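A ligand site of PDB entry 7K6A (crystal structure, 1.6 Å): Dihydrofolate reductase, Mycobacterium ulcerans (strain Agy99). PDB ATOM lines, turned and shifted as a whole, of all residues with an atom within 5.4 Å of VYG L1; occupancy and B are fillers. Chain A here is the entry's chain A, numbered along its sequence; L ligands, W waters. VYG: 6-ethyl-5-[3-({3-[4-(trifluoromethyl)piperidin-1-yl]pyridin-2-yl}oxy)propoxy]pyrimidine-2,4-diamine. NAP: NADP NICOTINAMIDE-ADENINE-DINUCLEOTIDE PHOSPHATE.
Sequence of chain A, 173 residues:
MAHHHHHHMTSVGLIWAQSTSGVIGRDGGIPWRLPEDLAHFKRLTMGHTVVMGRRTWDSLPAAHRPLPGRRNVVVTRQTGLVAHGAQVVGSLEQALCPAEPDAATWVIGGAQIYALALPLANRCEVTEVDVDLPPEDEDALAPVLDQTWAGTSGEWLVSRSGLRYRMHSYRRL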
ATOM      1  N   ILE A  15      29.938   5.464 -22.263  1.00  0.00           N
ATOM      2  CA  ILE A  15      29.730   4.714 -23.489  1.00  0.00           C
ATOM      3  C   ILE A  15      30.128   5.604 -24.657  1.00  0.00           C
ATOM      4  O   ILE A  15      29.740   6.781 -24.705  1.00  0.00           O
ATOM      5  CB  ILE A  15      28.266   4.212 -23.614  1.00  0.00           C
ATOM      6  CG1 ILE A  15      28.085   3.397 -24.897  1.00  0.00           C
ATOM      7  CG2 ILE A  15      27.278   5.384 -23.534  1.00  0.00           C
ATOM      8  CD1 ILE A  15      26.748   2.634 -24.951  1.00  0.00           C
ATOM      9  N   TRP A  16      30.973   5.074 -25.545  1.00  0.00           N
ATOM     10  CA  TRP A  16      31.436   5.843 -26.690  1.00  0.00           C
ATOM     11  C   TRP A  16      31.823   4.885 -27.803  1.00  0.00           C
ATOM     12  O   TRP A  16      32.039   3.686 -27.578  1.00  0.00           O
ATOM     13  CB  TRP A  16      32.625   6.733 -26.337  1.00  0.00           C
ATOM     14  CG  TRP A  16      33.988   6.094 -26.145  1.00  0.00           C
ATOM     15  CD1 TRP A  16      34.922   5.810 -27.117  1.00  0.00           C
ATOM     16  CD2 TRP A  16      34.605   5.778 -24.889  1.00  0.00           C
ATOM     17  NE1 TRP A  16      36.063   5.292 -26.531  1.00  0.00           N
ATOM     18  CE2 TRP A  16      35.887   5.265 -25.168  1.00  0.00           C
ATOM     19  CE3 TRP A  16      34.181   5.853 -23.554  1.00  0.00           C
ATOM     20  CZ2 TRP A  16      36.765   4.839 -24.161  1.00  0.00           C
ATOM     21  CZ3 TRP A  16      35.042   5.419 -22.558  1.00  0.00           C
ATOM     22  CH2 TRP A  16      36.322   4.913 -22.867  1.00  0.00           C
ATOM     23  N   ALA A  17      31.895   5.437 -29.009  1.00  0.00           N
ATOM     24  CA  ALA A  17      32.425   4.750 -30.183  1.00  0.00           C
ATOM     25  C   ALA A  17      33.625   5.527 -30.703  1.00  0.00           C
ATOM     26  O   ALA A  17      33.602   6.751 -30.778  1.00  0.00           O
ATOM     27  CB  ALA A  17      31.354   4.618 -31.269  1.00  0.00           C
ATOM     28  N   ILE A  30      29.972  12.757 -35.810  1.00  0.00           N
ATOM     29  CA  ILE A  30      30.718  11.504 -35.722  1.00  0.00           C
ATOM     30  C   ILE A  30      31.104  11.114 -37.154  1.00  0.00           C
ATOM     31  O   ILE A  30      30.208  10.966 -38.006  1.00  0.00           O
ATOM     32  CB  ILE A  30      29.915  10.396 -35.044  1.00  0.00           C
ATOM     33  CG1 ILE A  30      29.616  10.766 -33.570  1.00  0.00           C
ATOM     34  CG2 ILE A  30      30.677   9.070 -35.106  1.00  0.00           C
ATOM     35  CD1 ILE A  30      28.711   9.755 -32.846  1.00  0.00           C
ATOM     36  N   ASP A  37      26.423   0.117 -34.208  1.00  0.00           N
ATOM     37  CA  ASP A  37      26.756   0.872 -33.006  1.00  0.00           C
ATOM     38  C   ASP A  37      25.553   1.670 -32.506  1.00  0.00           C
ATOM     39  O   ASP A  37      25.306   1.730 -31.284  1.00  0.00           O
ATOM     40  CB  ASP A  37      27.908   1.829 -33.261  1.00  0.00           C
ATOM     41  CG  ASP A  37      28.168   2.697 -32.063  1.00  0.00           C
ATOM     42  OD1 ASP A  37      28.605   2.137 -31.046  1.00  0.00           O
ATOM     43  OD2 ASP A  37      27.886   3.911 -32.118  1.00  0.00           O
ATOM     44  N   LEU A  38      24.817   2.304 -33.412  1.00  0.00           N
ATOM     45  CA  LEU A  38      23.612   3.012 -32.982  1.00  0.00           C
ATOM     46  C   LEU A  38      22.668   2.071 -32.252  1.00  0.00           C
ATOM     47  O   LEU A  38      22.109   2.430 -31.198  1.00  0.00           O
ATOM     48  CB  LEU A  38      22.901   3.636 -34.178  1.00  0.00           C
ATOM     49  CG  LEU A  38      23.228   5.102 -34.441  1.00  0.00           C
ATOM     50  CD1 LEU A  38      24.673   5.223 -34.971  1.00  0.00           C
ATOM     51  CD2 LEU A  38      22.233   5.755 -35.394  1.00  0.00           C
ATOM     52  N   HIS A  40      23.391  -0.786 -30.665  1.00  0.00           N
ATOM     53  CA  HIS A  40      24.050  -1.115 -29.403  1.00  0.00           C
ATOM     54  C   HIS A  40      23.828  -0.010 -28.368  1.00  0.00           C
ATOM     55  O   HIS A  40      23.395  -0.269 -27.227  1.00  0.00           O
ATOM     56  CB  HIS A  40      25.537  -1.332 -29.699  1.00  0.00           C
ATOM     57  CG  HIS A  40      26.424  -1.505 -28.506  1.00  0.00           C
ATOM     58  ND1 HIS A  40      26.390  -2.617 -27.709  1.00  0.00           N
ATOM     59  CD2 HIS A  40      27.425  -0.726 -28.035  1.00  0.00           C
ATOM     60  CE1 HIS A  40      27.318  -2.517 -26.776  1.00  0.00           C
ATOM     61  NE2 HIS A  40      27.962  -1.375 -26.949  1.00  0.00           N
ATOM     62  N   PHE A  41      24.130   1.224 -28.751  1.00  0.00           N
ATOM     63  CA  PHE A  41      23.913   2.385 -27.889  1.00  0.00           C
ATOM     64  C   PHE A  41      22.452   2.516 -27.468  1.00  0.00           C
ATOM     65  O   PHE A  41      22.154   2.760 -26.297  1.00  0.00           O
ATOM     66  CB  PHE A  41      24.381   3.653 -28.610  1.00  0.00           C
ATOM     67  CG  PHE A  41      24.048   4.914 -27.854  1.00  0.00           C
ATOM     68  CD1 PHE A  41      24.907   5.385 -26.869  1.00  0.00           C
ATOM     69  CD2 PHE A  41      22.869   5.622 -28.100  1.00  0.00           C
ATOM     70  CE1 PHE A  41      24.631   6.548 -26.157  1.00  0.00           C
ATOM     71  CE2 PHE A  41      22.562   6.780 -27.388  1.00  0.00           C
ATOM     72  CZ  PHE A  41      23.447   7.245 -26.416  1.00  0.00           C
ATOM     73  N   LYS A  42      21.522   2.361 -28.423  1.00  0.00           N
ATOM     74  CA  LYS A  42      20.098   2.483 -28.119  1.00  0.00           C
ATOM     75  C   LYS A  42      19.661   1.452 -27.093  1.00  0.00           C
ATOM     76  O   LYS A  42      18.962   1.787 -26.120  1.00  0.00           O
ATOM     77  CB  LYS A  42      19.267   2.357 -29.399  1.00  0.00           C
ATOM     78  CG  LYS A  42      19.269   3.633 -30.221  1.00  0.00           C
ATOM     79  CD  LYS A  42      18.927   3.434 -31.713  1.00  0.00           C
ATOM     80  CE  LYS A  42      17.452   3.372 -31.988  1.00  0.00           C
ATOM     81  NZ  LYS A  42      17.191   3.461 -33.463  1.00  0.00           N
ATOM     82  N   THR A  45      21.051   2.096 -23.423  1.00  0.00           N
ATOM     83  CA  THR A  45      20.678   3.313 -22.725  1.00  0.00           C
ATOM     84  C   THR A  45      19.177   3.533 -22.571  1.00  0.00           C
ATOM     85  O   THR A  45      18.792   4.405 -21.784  1.00  0.00           O
ATOM     86  CB  THR A  45      21.269   4.559 -23.406  1.00  0.00           C
ATOM     87  OG1 THR A  45      20.778   4.697 -24.747  1.00  0.00           O
ATOM     88  CG2 THR A  45      22.803   4.510 -23.412  1.00  0.00           C
ATOM     89  N   THR A  56      27.760  18.074 -27.273  1.00  0.00           N
ATOM     90  CA  THR A  56      27.101  16.856 -27.751  1.00  0.00           C
ATOM     91  C   THR A  56      25.593  17.039 -27.850  1.00  0.00           C
ATOM     92  O   THR A  56      24.977  16.581 -28.812  1.00  0.00           O
ATOM     93  CB  THR A  56      27.478  15.687 -26.831  1.00  0.00           C
ATOM     94  OG1 THR A  56      28.855  15.405 -27.013  1.00  0.00           O
ATOM     95  CG2 THR A  56      26.655  14.436 -27.165  1.00  0.00           C
ATOM     96  N   SER A  59      24.947  18.603 -31.008  1.00  0.00           N
ATOM     97  CA  SER A  59      25.283  17.765 -32.154  1.00  0.00           C
ATOM     98  C   SER A  59      24.199  16.742 -32.490  1.00  0.00           C
ATOM     99  O   SER A  59      24.285  16.118 -33.549  1.00  0.00           O
ATOM    100  CB  SER A  59      26.603  17.006 -31.904  1.00  0.00           C
ATOM    101  OG  SER A  59      26.379  15.899 -31.036  1.00  0.00           O
ATOM    102  N   LEU A  60      23.186  16.603 -31.646  1.00  0.00           N
ATOM    103  CA  LEU A  60      22.236  15.502 -31.830  1.00  0.00           C
ATOM    104  C   LEU A  60      21.377  15.713 -33.067  1.00  0.00           C
ATOM    105  O   LEU A  60      20.931  16.840 -33.338  1.00  0.00           O
ATOM    106  CB  LEU A  60      21.339  15.371 -30.600  1.00  0.00           C
ATOM    107  CG  LEU A  60      22.012  14.926 -29.312  1.00  0.00           C
ATOM    108  CD1 LEU A  60      21.062  15.129 -28.132  1.00  0.00           C
ATOM    109  CD2 LEU A  60      22.439  13.471 -29.428  1.00  0.00           C
ATOM    110  N   PRO A  61      21.096  14.657 -33.824  1.00  0.00           N
ATOM    111  CA  PRO A  61      20.109  14.769 -34.903  1.00  0.00           C
ATOM    112  C   PRO A  61      18.780  15.247 -34.343  1.00  0.00           C
ATOM    113  O   PRO A  61      18.412  14.932 -33.206  1.00  0.00           O
ATOM    114  CB  PRO A  61      20.009  13.330 -35.442  1.00  0.00           C
ATOM    115  CG  PRO A  61      21.278  12.658 -34.987  1.00  0.00           C
ATOM    116  CD  PRO A  61      21.651  13.308 -33.687  1.00  0.00           C
ATOM    117  N   HIS A  64      16.423  13.080 -32.451  1.00  0.00           N
ATOM    118  CA  HIS A  64      16.908  12.504 -31.204  1.00  0.00           C
ATOM    119  C   HIS A  64      17.380  13.581 -30.236  1.00  0.00           C
ATOM    120  O   HIS A  64      18.248  13.344 -29.404  1.00  0.00           O
ATOM    121  CB  HIS A  64      18.021  11.485 -31.482  1.00  0.00           C
ATOM    122  CG  HIS A  64      17.532  10.232 -32.149  1.00  0.00           C
ATOM    123  ND1 HIS A  64      17.994   9.802 -33.377  1.00  0.00           N
ATOM    124  CD2 HIS A  64      16.588   9.339 -31.766  1.00  0.00           C
ATOM    125  CE1 HIS A  64      17.371   8.687 -33.712  1.00  0.00           C
ATOM    126  NE2 HIS A  64      16.522   8.377 -32.748  1.00  0.00           N
ATOM    127  N   LEU A  67      16.955  12.697 -26.558  1.00  0.00           N
ATOM    128  CA  LEU A  67      16.893  11.252 -26.793  1.00  0.00           C
ATOM    129  C   LEU A  67      15.589  10.718 -26.206  1.00  0.00           C
ATOM    130  O   LEU A  67      15.309  10.971 -25.034  1.00  0.00           O
ATOM    131  CB  LEU A  67      18.095  10.515 -26.175  1.00  0.00           C
ATOM    132  CG  LEU A  67      19.429  10.677 -26.896  1.00  0.00           C
ATOM    133  CD1 LEU A  67      20.102  11.987 -26.521  1.00  0.00           C
ATOM    134  CD2 LEU A  67      20.328   9.489 -26.576  1.00  0.00           C
ATOM    135  N   PRO A  68      14.767  10.007 -26.987  1.00  0.00           N
ATOM    136  CA  PRO A  68      13.474   9.569 -26.482  1.00  0.00           C
ATOM    137  C   PRO A  68      13.613   8.484 -25.441  1.00  0.00           C
ATOM    138  O   PRO A  68      14.514   7.638 -25.519  1.00  0.00           O
ATOM    139  CB  PRO A  68      12.762   9.033 -27.732  1.00  0.00           C
ATOM    140  CG  PRO A  68      13.919   8.604 -28.653  1.00  0.00           C
ATOM    141  CD  PRO A  68      14.923   9.725 -28.426  1.00  0.00           C
ATOM    142  N   ARG A  70      14.519   8.386 -22.410  1.00  0.00           N
ATOM    143  CA  ARG A  70      15.708   8.458 -21.577  1.00  0.00           C
ATOM    144  C   ARG A  70      15.658   9.791 -20.849  1.00  0.00           C
ATOM    145  O   ARG A  70      15.111  10.760 -21.385  1.00  0.00           O
ATOM    146  CB  ARG A  70      16.970   8.351 -22.423  1.00  0.00           C
ATOM    147  CG  ARG A  70      17.087   7.003 -23.178  1.00  0.00           C
ATOM    148  CD  ARG A  70      18.078   7.118 -24.313  1.00  0.00           C
ATOM    149  NE  ARG A  70      18.225   5.887 -25.096  1.00  0.00           N
ATOM    150  CZ  ARG A  70      17.519   5.610 -26.188  1.00  0.00           C
ATOM    151  NH1 ARG A  70      16.613   6.456 -26.663  1.00  0.00           N
ATOM    152  NH2 ARG A  70      17.748   4.461 -26.824  1.00  0.00           N
ATOM    153  N   VAL A 107      27.125   8.186 -19.241  1.00  0.00           N
ATOM    154  CA  VAL A 107      27.713   9.416 -19.761  1.00  0.00           C
ATOM    155  C   VAL A 107      27.970   9.166 -21.249  1.00  0.00           C
ATOM    156  O   VAL A 107      28.677   8.233 -21.613  1.00  0.00           O
ATOM    157  CB  VAL A 107      28.991   9.775 -18.993  1.00  0.00           C
ATOM    158  CG1 VAL A 107      29.748  10.926 -19.670  1.00  0.00           C
ATOM    159  CG2 VAL A 107      28.634  10.149 -17.525  1.00  0.00           C
ATOM    160  N   ILE A 108      27.347   9.983 -22.111  1.00  0.00           N
ATOM    161  CA  ILE A 108      27.309   9.658 -23.540  1.00  0.00           C
ATOM    162  C   ILE A 108      28.135  10.641 -24.380  1.00  0.00           C
ATOM    163  O   ILE A 108      27.981  10.649 -25.610  1.00  0.00           O
ATOM    164  CB  ILE A 108      25.870   9.583 -24.066  1.00  0.00           C
ATOM    165  CG1 ILE A 108      25.154  10.951 -24.018  1.00  0.00           C
ATOM    166  CG2 ILE A 108      25.053   8.550 -23.290  1.00  0.00           C
ATOM    167  CD1 ILE A 108      23.862  10.963 -24.859  1.00  0.00           C
ATOM    168  N   GLY A 109      28.993  11.434 -23.766  1.00  0.00           N
ATOM    169  CA  GLY A 109      29.960  12.285 -24.455  1.00  0.00           C
ATOM    170  C   GLY A 109      29.755  13.750 -24.153  1.00  0.00           C
ATOM    171  O   GLY A 109      28.830  14.138 -23.445  1.00  0.00           O
ATOM    172  N   TYR A 114      33.664  13.216 -21.000  1.00  0.00           N
ATOM    173  CA  TYR A 114      34.242  11.919 -20.638  1.00  0.00           C
ATOM    174  C   TYR A 114      35.409  12.100 -19.678  1.00  0.00           C
ATOM    175  O   TYR A 114      35.585  11.298 -18.752  1.00  0.00           O
ATOM    176  CB  TYR A 114      34.748  11.134 -21.852  1.00  0.00           C
ATOM    177  CG  TYR A 114      33.698  10.585 -22.763  1.00  0.00           C
ATOM    178  CD1 TYR A 114      32.552   9.963 -22.273  1.00  0.00           C
ATOM    179  CD2 TYR A 114      33.843  10.694 -24.149  1.00  0.00           C
ATOM    180  CE1 TYR A 114      31.592   9.454 -23.138  1.00  0.00           C
ATOM    181  CE2 TYR A 114      32.868  10.212 -25.018  1.00  0.00           C
ATOM    182  CZ  TYR A 114      31.759   9.583 -24.510  1.00  0.00           C
ATOM    183  OH  TYR A 114      30.815   9.107 -25.379  1.00  0.00           O
ATOM    184  N   GLU A 125      31.694   1.192 -21.884  1.00  0.00           N
ATOM    185  CA  GLU A 125      31.277   0.374 -23.024  1.00  0.00           C
ATOM    186  C   GLU A 125      31.765   1.071 -24.299  1.00  0.00           C
ATOM    187  O   GLU A 125      31.296   2.163 -24.627  1.00  0.00           O
ATOM    188  CB  GLU A 125      29.762   0.199 -23.016  1.00  0.00           C
ATOM    189  CG  GLU A 125      29.227  -0.613 -21.815  1.00  0.00           C
ATOM    190  CD  GLU A 125      29.675  -2.080 -21.832  1.00  0.00           C
ATOM    191  OE1 GLU A 125      29.974  -2.585 -22.936  1.00  0.00           O
ATOM    192  OE2 GLU A 125      29.719  -2.723 -20.753  1.00  0.00           O
ATOM    193  N   THR A 127      32.775   0.986 -28.425  1.00  0.00           N
ATOM    194  CA  THR A 127      32.770   0.402 -29.769  1.00  0.00           C
ATOM    195  C   THR A 127      34.013   0.876 -30.490  1.00  0.00           C
ATOM    196  O   THR A 127      34.283   2.083 -30.539  1.00  0.00           O
ATOM    197  CB  THR A 127      31.523   0.823 -30.545  1.00  0.00           C
ATOM    198  OG1 THR A 127      30.369   0.471 -29.781  1.00  0.00           O
ATOM    199  CG2 THR A 127      31.442   0.108 -31.913  1.00  0.00           C
HETATM  200  C1  VYG L   1      26.655   7.258 -31.366  1.00  0.00           C
HETATM  201  C2  VYG L   1      27.220   6.779 -30.040  1.00  0.00           C
HETATM  202  C3  VYG L   1      28.112   5.062 -28.800  1.00  0.00           C
HETATM  203  C4  VYG L   1      27.894   7.060 -27.768  1.00  0.00           C
HETATM  204  C5  VYG L   1      27.336   7.593 -28.960  1.00  0.00           C
HETATM  205  C6  VYG L   1      25.628   9.235 -28.471  1.00  0.00           C
HETATM  206  C7  VYG L   1      25.569  10.770 -28.508  1.00  0.00           C
HETATM  207  N1  VYG L   1      28.506   3.767 -28.736  1.00  0.00           N
HETATM  208  C8  VYG L   1      25.703  11.281 -29.939  1.00  0.00           C
HETATM  209  C9  VYG L   1      24.653  10.793 -32.086  1.00  0.00           C
HETATM  210  C10 VYG L   1      25.613  11.591 -33.994  1.00  0.00           C
HETATM  211  C11 VYG L   1      24.679  10.959 -34.775  1.00  0.00           C
HETATM  212  N2  VYG L   1      28.273   5.789 -27.688  1.00  0.00           N
HETATM  213  C12 VYG L   1      23.683  10.192 -34.158  1.00  0.00           C
HETATM  214  C13 VYG L   1      23.646  10.075 -32.779  1.00  0.00           C
HETATM  215  C14 VYG L   1      21.922   8.350 -32.858  1.00  0.00           C
HETATM  216  C15 VYG L   1      21.082   7.463 -31.916  1.00  0.00           C
HETATM  217  C16 VYG L   1      20.149   8.322 -31.036  1.00  0.00           C
HETATM  218  C17 VYG L   1      19.300   7.496 -30.121  1.00  0.00           C
HETATM  219  C18 VYG L   1      21.012   9.263 -30.196  1.00  0.00           C
HETATM  220  C19 VYG L   1      21.784  10.138 -31.199  1.00  0.00           C
HETATM  221  O1  VYG L   1      24.642  10.693 -30.715  1.00  0.00           O
HETATM  222  N3  VYG L   1      28.021   7.832 -26.676  1.00  0.00           N
HETATM  223  N   VYG L   1      27.636   5.503 -29.953  1.00  0.00           N
HETATM  224  C   VYG L   1      25.270   6.629 -31.604  1.00  0.00           C
HETATM  225  O   VYG L   1      26.978   8.940 -28.962  1.00  0.00           O
HETATM  226  F   VYG L   1      18.499   8.253 -29.340  1.00  0.00           F
HETATM  227  F1  VYG L   1      20.041   6.719 -29.297  1.00  0.00           F
HETATM  228  F2  VYG L   1      18.517   6.661 -30.829  1.00  0.00           F
HETATM  229  N4  VYG L   1      25.568  11.513 -32.648  1.00  0.00           N
HETATM  230  N5  VYG L   1      22.669   9.347 -32.084  1.00  0.00           N
HETATM  231  PA  NAP L   2      31.221  17.986 -25.080  1.00  0.00           P
HETATM  232  O1A NAP L   2      30.037  17.251 -25.574  1.00  0.00           O
HETATM  233  O2A NAP L   2      32.063  17.290 -24.058  1.00  0.00           O
HETATM  234  O5B NAP L   2      30.643  19.405 -24.484  1.00  0.00           O
HETATM  235  C5B NAP L   2      31.558  20.434 -24.078  1.00  0.00           C
HETATM  236  C4B NAP L   2      30.767  21.447 -23.314  1.00  0.00           C
HETATM  237  O4B NAP L   2      30.388  20.903 -22.032  1.00  0.00           O
HETATM  238  C3B NAP L   2      31.543  22.724 -23.003  1.00  0.00           C
HETATM  239  O3B NAP L   2      31.581  23.600 -24.127  1.00  0.00           O
HETATM  240  C2B NAP L   2      30.690  23.232 -21.843  1.00  0.00           C
HETATM  241  O2B NAP L   2      29.419  23.742 -22.312  1.00  0.00           O
HETATM  242  C1B NAP L   2      30.408  21.953 -21.081  1.00  0.00           C
HETATM  243  N9A NAP L   2      31.401  21.670 -20.060  1.00  0.00           N
HETATM  244  C8A NAP L   2      32.661  21.157 -20.194  1.00  0.00           C
HETATM  245  N7A NAP L   2      33.342  21.099 -19.080  1.00  0.00           N
HETATM  246  C5A NAP L   2      32.473  21.602 -18.135  1.00  0.00           C
HETATM  247  C6A NAP L   2      32.582  21.825 -16.752  1.00  0.00           C
HETATM  248  N6A NAP L   2      33.682  21.512 -16.038  1.00  0.00           N
HETATM  249  N1A NAP L   2      31.522  22.361 -16.098  1.00  0.00           N
HETATM  250  C2A NAP L   2      30.423  22.650 -16.807  1.00  0.00           C
HETATM  251  N3A NAP L   2      30.198  22.484 -18.112  1.00  0.00           N
HETATM  252  C4A NAP L   2      31.259  21.961 -18.722  1.00  0.00           C
HETATM  253  O3  NAP L   2      32.128  18.494 -26.291  1.00  0.00           O
HETATM  254  PN  NAP L   2      33.275  17.831 -27.190  1.00  0.00           P
HETATM  255  O1N NAP L   2      34.329  17.268 -26.323  1.00  0.00           O
HETATM  256  O2N NAP L   2      33.641  18.845 -28.217  1.00  0.00           O
HETATM  257  O5D NAP L   2      32.524  16.620 -27.867  1.00  0.00           O
HETATM  258  C5D NAP L   2      31.583  16.796 -28.954  1.00  0.00           C
HETATM  259  C4D NAP L   2      32.084  16.015 -30.147  1.00  0.00           C
HETATM  260  O4D NAP L   2      32.147  14.603 -29.828  1.00  0.00           O
HETATM  261  C3D NAP L   2      31.191  16.103 -31.389  1.00  0.00           C
HETATM  262  O3D NAP L   2      31.977  15.971 -32.568  1.00  0.00           O
HETATM  263  C2D NAP L   2      30.285  14.895 -31.219  1.00  0.00           C
HETATM  264  O2D NAP L   2      29.702  14.497 -32.446  1.00  0.00           O
HETATM  265  C1D NAP L   2      31.291  13.882 -30.692  1.00  0.00           C
HETATM  266  N1N NAP L   2      30.667  12.744 -29.906  1.00  0.00           N
HETATM  267  C2N NAP L   2      31.048  11.506 -30.250  1.00  0.00           C
HETATM  268  C3N NAP L   2      30.618  10.418 -29.512  1.00  0.00           C
HETATM  269  C7N NAP L   2      31.032   9.021 -29.901  1.00  0.00           C
HETATM  270  O7N NAP L   2      30.779   8.082 -29.119  1.00  0.00           O
HETATM  271  N7N NAP L   2      31.712   8.868 -31.039  1.00  0.00           N
HETATM  272  C4N NAP L   2      29.766  10.642 -28.433  1.00  0.00           C
HETATM  273  C5N NAP L   2      29.372  11.928 -28.120  1.00  0.00           C
HETATM  274  C6N NAP L   2      29.831  12.988 -28.875  1.00  0.00           C
HETATM  275  P2B NAP L   2      29.186  25.327 -22.525  1.00  0.00           P
HETATM  276  O1X NAP L   2      29.526  25.994 -21.230  1.00  0.00           O
HETATM  277  O2X NAP L   2      30.092  25.721 -23.658  1.00  0.00           O
HETATM  278  O3X NAP L   2      27.714  25.413 -22.872  1.00  0.00           O
HETATM  279  O   HOH W   1      29.779   1.433 -27.154  1.00  0.00           O
HETATM  280  O   HOH W   2      27.376  13.546 -31.790  1.00  0.00           O
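NE2 of His 64 lies close to F2 of VYG L1. Residues that only touch VYG L1: Trp 16, Ala 17, Ile 30, Leu 38, Phe 41, Lys 42, Leu 60, Pro 61, Leu 67, Pro 68, Arg 70 and Thr 127. Hydrophobic or aromatic side chains within 4 Å of VYG L1: Ile 15, Ala 17, Ile 30, Leu 38, Phe 41, Leu 60, Pro 61, His 64, Leu 67, Pro 68 and Ile 108. Of the 24 residues printed, 17 come within 4 Å of VYG L1. The nearest printed residue that does not touch VYG L1 is Thr 56 (4.1 Å).
Water W2 lies within hydrogen-bond range of O2D of NAP L2 (2.6 Å), OG of Ser 59 (2.7 Å) and N4 of VYG L1 (2.9 Å). Water W1 lies within hydrogen-bond range of the side-chain hydroxyl of Thr 127 (2.9 Å), the backbone carbonyl oxygen of Glu 125 (3.0 Å), a nitrogen (N1) of VYG L1 (3.1 Å), the backbone carbonyl oxygen of Trp 16 (3.2 Å) and a ring nitrogen (NE2) of His 40 (3.4 Å).
The side-chain hydroxyl (OH) of Tyr 114 sits at hydrogen-bond distance from the backbone carbonyl oxygen (O) of Ile 15 (2.6 Å). O of Trp 16 is in hydrogen-bond range of N of Thr 127, 2.9 Å away. O of Lys 42 is in hydrogen-bond range of NH2 of Arg 70, at 3.0 Å. The side-chain hydroxyl (OH) of Tyr 114 lies close to the backbone NH (N) of Gly 109, 3.4 Å away. NH1 of Arg 70 is in hydrogen-bond range of O of Pro 68 (2.7 Å). O of Glu 125 is in hydrogen-bond range of N of Trp 16, at 3.1 Å. The backbone carbonyl oxygen (O) of Val 107 is in hydrogen-bond range of the backbone NH (N) of Ile 15, 3.1 Å away. The side-chain carboxylate of Asp 37 is in hydrogen-bond range of the side-chain hydroxyl of Thr 127.
An oxygen (O1A) of NAP L2 is in hydrogen-bond range of the backbone NH of Thr 56, 3.0 Å away. The side-chain carboxylate (OD2) of Asp 37 is in hydrogen-bond range of a nitrogen (N) of VYG L1. O of Ala 17 sits at hydrogen-bond distance from N7N of NAP L2 (2.8 Å). OG1 of Thr 56 sits at hydrogen-bond distance from O1A of NAP L2 (2.6 Å). A nitrogen (N3) of VYG L1 sits at hydrogen-bond distance from the side-chain hydroxyl (OH) of Tyr 114 (3.3 Å). N3 of VYG L1 lies within hydrogen-bond range of O of Ile 15 (2.8 Å). N of Ala 17 sits at hydrogen-bond distance from O7N of NAP L2, 2.9 Å away. A nitrogen (N3) of VYG L1 is in hydrogen-bond range of the backbone carbonyl oxygen (O) of Ile 108 (3.0 Å).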
